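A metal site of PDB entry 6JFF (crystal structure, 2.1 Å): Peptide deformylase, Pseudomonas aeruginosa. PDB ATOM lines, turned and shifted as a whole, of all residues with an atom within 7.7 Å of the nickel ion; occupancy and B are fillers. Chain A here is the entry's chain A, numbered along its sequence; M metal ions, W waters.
Water W2 bridges the side-chain carboxylate of Glu 143 (2.5 Å) and the side-chain amide oxygen of Gln 52 (2.9 Å).
SG of Cys 100 lies close to N of Ser 102 (3.7 Å). The side-chain amide oxygen of Gln 52 sits close to a ring nitrogen (NE2) of His 146 (3.5 Å). A ring nitrogen (ND1) of His 142 sits at hydrogen-bond distance from the side-chain carboxylate (OE1) of Glu 98 (2.6 Å). The side-chain amide oxygen (OE1) of Gln 52 lies within hydrogen-bond range of the backbone NH (N) of Ala 49, 2.8 Å away. The side-chain hydroxyl (OG) of Ser 102 is in hydrogen-bond range of the side-chain amide nitrogen (NE2) of Gln 52 (3.0 Å). SG of Cys 100 lies close to NE2 of Gln 52, 3.6 Å away.
The nickel ion is bound by a ring nitrogen (NE2) of His 146, the side-chain sulfur (SG) of Cys 100, water W2 and a ring nitrogen (NE2) of His 142.
Residues that only touch the nickel ion: Gln 52 (3.5 Å). Of the 19 residues printed, 4 come within 4 Å of the nickel ion.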
ATOM      1  N   GLY A  47       0.870  30.185  23.618  1.00  0.00           N
ATOM      2  CA  GLY A  47       0.420  28.814  23.723  1.00  0.00           C
ATOM      3  C   GLY A  47       1.066  27.935  22.654  1.00  0.00           C
ATOM      4  O   GLY A  47       1.602  28.450  21.680  1.00  0.00           O
ATOM      5  N   LEU A  48       1.010  26.624  22.824  1.00  0.00           N
ATOM      6  CA  LEU A  48       1.490  25.730  21.797  1.00  0.00           C
ATOM      7  C   LEU A  48       0.818  24.379  21.977  1.00  0.00           C
ATOM      8  O   LEU A  48       0.659  23.922  23.105  1.00  0.00           O
ATOM      9  CB  LEU A  48       3.001  25.619  21.910  1.00  0.00           C
ATOM     10  CG  LEU A  48       3.762  24.863  20.863  1.00  0.00           C
ATOM     11  CD1 LEU A  48       3.784  25.660  19.571  1.00  0.00           C
ATOM     12  CD2 LEU A  48       5.182  24.637  21.384  1.00  0.00           C
ATOM     13  N   ALA A  49       0.372  23.790  20.859  1.00  0.00           N
ATOM     14  CA  ALA A  49      -0.233  22.478  20.851  1.00  0.00           C
ATOM     15  C   ALA A  49       0.797  21.477  20.263  1.00  0.00           C
ATOM     16  O   ALA A  49       1.578  21.807  19.298  1.00  0.00           O
ATOM     17  CB  ALA A  49      -1.495  22.491  19.996  1.00  0.00           C
ATOM     18  N   GLN A  52       1.547  21.170  16.446  1.00  0.00           N
ATOM     19  CA  GLN A  52       2.320  22.208  15.779  1.00  0.00           C
ATOM     20  C   GLN A  52       3.835  21.881  15.743  1.00  0.00           C
ATOM     21  O   GLN A  52       4.588  22.513  15.016  1.00  0.00           O
ATOM     22  CB  GLN A  52       2.070  23.561  16.463  1.00  0.00           C
ATOM     23  CG  GLN A  52       0.620  24.052  16.514  1.00  0.00           C
ATOM     24  CD  GLN A  52       0.559  25.395  17.282  1.00  0.00           C
ATOM     25  OE1 GLN A  52       0.391  25.413  18.527  1.00  0.00           O
ATOM     26  NE2 GLN A  52       0.762  26.512  16.558  1.00  0.00           N
ATOM     27  N   GLU A  98      -6.381  37.354  17.197  1.00  0.00           N
ATOM     28  CA  GLU A  98      -5.585  36.175  17.375  1.00  0.00           C
ATOM     29  C   GLU A  98      -4.437  36.099  16.384  1.00  0.00           C
ATOM     30  O   GLU A  98      -4.479  36.646  15.281  1.00  0.00           O
ATOM     31  CB  GLU A  98      -6.486  34.938  17.261  1.00  0.00           C
ATOM     32  CG  GLU A  98      -7.547  34.819  18.375  1.00  0.00           C
ATOM     33  CD  GLU A  98      -8.256  33.455  18.419  1.00  0.00           C
ATOM     34  OE1 GLU A  98      -7.726  32.417  17.879  1.00  0.00           O
ATOM     35  OE2 GLU A  98      -9.343  33.408  18.976  1.00  0.00           O
ATOM     36  N   GLY A  99      -3.397  35.398  16.800  1.00  0.00           N
ATOM     37  CA  GLY A  99      -2.254  35.100  15.973  1.00  0.00           C
ATOM     38  C   GLY A  99      -1.855  33.693  16.384  1.00  0.00           C
ATOM     39  O   GLY A  99      -2.535  33.063  17.223  1.00  0.00           O
ATOM     40  N   CYS A 100      -0.752  33.192  15.843  1.00  0.00           N
ATOM     41  CA  CYS A 100      -0.399  31.795  16.002  1.00  0.00           C
ATOM     42  C   CYS A 100       0.982  31.602  15.328  1.00  0.00           C
ATOM     43  O   CYS A 100       1.238  32.079  14.210  1.00  0.00           O
ATOM     44  CB  CYS A 100      -1.464  30.993  15.269  1.00  0.00           C
ATOM     45  SG  CYS A 100      -1.256  29.209  15.285  1.00  0.00           S
ATOM     46  N   LEU A 101       1.853  30.860  15.965  1.00  0.00           N
ATOM     47  CA  LEU A 101       3.209  30.597  15.433  1.00  0.00           C
ATOM     48  C   LEU A 101       3.190  29.789  14.097  1.00  0.00           C
ATOM     49  O   LEU A 101       4.076  29.933  13.262  1.00  0.00           O
ATOM     50  CB  LEU A 101       4.027  29.905  16.524  1.00  0.00           C
ATOM     51  CG  LEU A 101       4.084  30.732  17.873  1.00  0.00           C
ATOM     52  CD1 LEU A 101       4.316  29.860  19.120  1.00  0.00           C
ATOM     53  CD2 LEU A 101       5.088  31.877  17.723  1.00  0.00           C
ATOM     54  N   SER A 102       2.140  28.994  13.871  1.00  0.00           N
ATOM     55  CA  SER A 102       1.983  28.263  12.619  1.00  0.00           C
ATOM     56  C   SER A 102       1.424  29.113  11.459  1.00  0.00           C
ATOM     57  O   SER A 102       1.267  28.595  10.332  1.00  0.00           O
ATOM     58  CB  SER A 102       1.054  27.061  12.839  1.00  0.00           C
ATOM     59  OG  SER A 102       1.637  26.178  13.755  1.00  0.00           O
ATOM     60  N   VAL A 103       1.107  30.379  11.736  1.00  0.00           N
ATOM     61  CA  VAL A 103       0.561  31.346  10.754  1.00  0.00           C
ATOM     62  C   VAL A 103       1.328  32.668  10.888  1.00  0.00           C
ATOM     63  O   VAL A 103       0.746  33.703  11.249  1.00  0.00           O
ATOM     64  CB  VAL A 103      -0.941  31.616  11.023  1.00  0.00           C
ATOM     65  CG1 VAL A 103      -1.607  32.301   9.831  1.00  0.00           C
ATOM     66  CG2 VAL A 103      -1.661  30.318  11.329  1.00  0.00           C
ATOM     67  N   ARG A 112     -15.099  33.861  19.711  1.00  0.00           N
ATOM     68  CA  ARG A 112     -15.113  32.671  20.532  1.00  0.00           C
ATOM     69  C   ARG A 112     -16.099  32.783  21.676  1.00  0.00           C
ATOM     70  O   ARG A 112     -16.582  33.873  22.009  1.00  0.00           O
ATOM     71  CB  ARG A 112     -13.752  32.469  21.149  1.00  0.00           C
ATOM     72  CG  ARG A 112     -12.555  32.515  20.217  1.00  0.00           C
ATOM     73  CD  ARG A 112     -12.242  31.116  19.732  1.00  0.00           C
ATOM     74  NE  ARG A 112     -10.961  31.083  19.029  1.00  0.00           N
ATOM     75  CZ  ARG A 112     -10.517  30.062  18.317  1.00  0.00           C
ATOM     76  NH1 ARG A 112     -11.172  28.906  18.296  1.00  0.00           N
ATOM     77  NH2 ARG A 112      -9.417  30.196  17.626  1.00  0.00           N
ATOM     78  N   VAL A 139      -7.668  31.619  24.788  1.00  0.00           N
ATOM     79  CA  VAL A 139      -6.394  30.849  24.590  1.00  0.00           C
ATOM     80  C   VAL A 139      -6.713  29.332  24.552  1.00  0.00           C
ATOM     81  O   VAL A 139      -6.275  28.604  23.642  1.00  0.00           O
ATOM     82  CB  VAL A 139      -5.397  31.171  25.709  1.00  0.00           C
ATOM     83  CG1 VAL A 139      -4.250  30.194  25.727  1.00  0.00           C
ATOM     84  CG2 VAL A 139      -4.831  32.566  25.516  1.00  0.00           C
ATOM     85  N   HIS A 142      -8.471  28.296  21.345  1.00  0.00           N
ATOM     86  CA  HIS A 142      -7.548  28.404  20.278  1.00  0.00           C
ATOM     87  C   HIS A 142      -6.599  27.191  20.262  1.00  0.00           C
ATOM     88  O   HIS A 142      -6.356  26.614  19.228  1.00  0.00           O
ATOM     89  CB  HIS A 142      -6.770  29.741  20.421  1.00  0.00           C
ATOM     90  CG  HIS A 142      -5.682  29.926  19.414  1.00  0.00           C
ATOM     91  ND1 HIS A 142      -5.765  30.832  18.384  1.00  0.00           N
ATOM     92  CD2 HIS A 142      -4.490  29.300  19.260  1.00  0.00           C
ATOM     93  CE1 HIS A 142      -4.652  30.781  17.663  1.00  0.00           C
ATOM     94  NE2 HIS A 142      -3.858  29.857  18.172  1.00  0.00           N
ATOM     95  N   GLU A 143      -6.053  26.841  21.391  1.00  0.00           N
ATOM     96  CA  GLU A 143      -5.119  25.700  21.434  1.00  0.00           C
ATOM     97  C   GLU A 143      -5.846  24.327  21.244  1.00  0.00           C
ATOM     98  O   GLU A 143      -5.324  23.420  20.568  1.00  0.00           O
ATOM     99  CB  GLU A 143      -4.358  25.672  22.772  1.00  0.00           C
ATOM    100  CG  GLU A 143      -3.330  26.727  22.941  1.00  0.00           C
ATOM    101  CD  GLU A 143      -2.393  26.911  21.779  1.00  0.00           C
ATOM    102  OE1 GLU A 143      -1.764  25.869  21.328  1.00  0.00           O
ATOM    103  OE2 GLU A 143      -2.252  28.099  21.348  1.00  0.00           O
ATOM    104  N   ASP A 145      -8.362  23.884  19.454  1.00  0.00           N
ATOM    105  CA  ASP A 145      -8.611  23.807  17.971  1.00  0.00           C
ATOM    106  C   ASP A 145      -7.497  23.118  17.228  1.00  0.00           C
ATOM    107  O   ASP A 145      -7.747  22.372  16.310  1.00  0.00           O
ATOM    108  CB  ASP A 145      -8.854  25.162  17.322  1.00  0.00           C
ATOM    109  CG  ASP A 145     -10.333  25.515  17.228  1.00  0.00           C
ATOM    110  OD1 ASP A 145     -11.168  24.628  17.501  1.00  0.00           O
ATOM    111  OD2 ASP A 145     -10.646  26.675  16.867  1.00  0.00           O
ATOM    112  N   HIS A 146      -6.278  23.295  17.668  1.00  0.00           N
ATOM    113  CA  HIS A 146      -5.202  22.524  17.036  1.00  0.00           C
ATOM    114  C   HIS A 146      -5.361  21.040  17.159  1.00  0.00           C
ATOM    115  O   HIS A 146      -4.816  20.334  16.354  1.00  0.00           O
ATOM    116  CB  HIS A 146      -3.865  22.859  17.642  1.00  0.00           C
ATOM    117  CG  HIS A 146      -3.399  24.201  17.296  1.00  0.00           C
ATOM    118  ND1 HIS A 146      -3.128  24.565  16.006  1.00  0.00           N
ATOM    119  CD2 HIS A 146      -3.123  25.297  18.062  1.00  0.00           C
ATOM    120  CE1 HIS A 146      -2.667  25.807  15.982  1.00  0.00           C
ATOM    121  NE2 HIS A 146      -2.684  26.278  17.212  1.00  0.00           N
ATOM    122  N   ARG A 150      -7.742  22.424  13.398  1.00  0.00           N
ATOM    123  CA  ARG A 150      -8.297  23.757  13.021  1.00  0.00           C
ATOM    124  C   ARG A 150      -7.343  24.823  13.370  1.00  0.00           C
ATOM    125  O   ARG A 150      -6.945  24.938  14.549  1.00  0.00           O
ATOM    126  CB  ARG A 150      -9.585  24.034  13.786  1.00  0.00           C
ATOM    127  CG  ARG A 150     -10.740  23.163  13.382  1.00  0.00           C
ATOM    128  CD  ARG A 150     -11.139  23.401  11.924  1.00  0.00           C
ATOM    129  NE  ARG A 150     -12.552  23.493  11.994  1.00  0.00           N
ATOM    130  CZ  ARG A 150     -13.281  24.584  11.879  1.00  0.00           C
ATOM    131  NH1 ARG A 150     -14.575  24.462  12.064  1.00  0.00           N
ATOM    132  NH2 ARG A 150     -12.778  25.746  11.555  1.00  0.00           N
ATOM    133  N   LEU A 151      -7.004  25.661  12.398  1.00  0.00           N
ATOM    134  CA  LEU A 151      -6.291  26.906  12.610  1.00  0.00           C
ATOM    135  C   LEU A 151      -7.261  28.064  12.515  1.00  0.00           C
ATOM    136  O   LEU A 151      -8.358  27.918  11.946  1.00  0.00           O
ATOM    137  CB  LEU A 151      -5.198  27.031  11.628  1.00  0.00           C
ATOM    138  CG  LEU A 151      -4.197  25.892  11.589  1.00  0.00           C
ATOM    139  CD1 LEU A 151      -3.058  26.250  10.669  1.00  0.00           C
ATOM    140  CD2 LEU A 151      -3.631  25.595  12.943  1.00  0.00           C
ATOM    141  N   TYR A 152      -6.893  29.190  13.125  1.00  0.00           N
ATOM    142  CA  TYR A 152      -7.850  30.302  13.336  1.00  0.00           C
ATOM    143  C   TYR A 152      -8.434  30.933  12.068  1.00  0.00           C
ATOM    144  O   TYR A 152      -9.616  31.278  12.060  1.00  0.00           O
ATOM    145  CB  TYR A 152      -7.323  31.350  14.311  1.00  0.00           C
ATOM    146  CG  TYR A 152      -6.346  32.284  13.726  1.00  0.00           C
ATOM    147  CD1 TYR A 152      -6.792  33.408  12.999  1.00  0.00           C
ATOM    148  CD2 TYR A 152      -5.008  32.074  13.869  1.00  0.00           C
ATOM    149  CE1 TYR A 152      -5.880  34.261  12.397  1.00  0.00           C
ATOM    150  CE2 TYR A 152      -4.085  32.905  13.268  1.00  0.00           C
ATOM    151  CZ  TYR A 152      -4.535  34.036  12.556  1.00  0.00           C
ATOM    152  OH  TYR A 152      -3.630  34.883  11.996  1.00  0.00           O
HETATM  153 NI    NI M   1      -2.116  28.354  17.282  1.00  0.00          NI
HETATM  154  O   HOH W   1      -4.622  28.741  14.900  1.00  0.00           O
HETATM  155  O   HOH W   2      -0.920  27.901  19.262  1.00  0.00           O
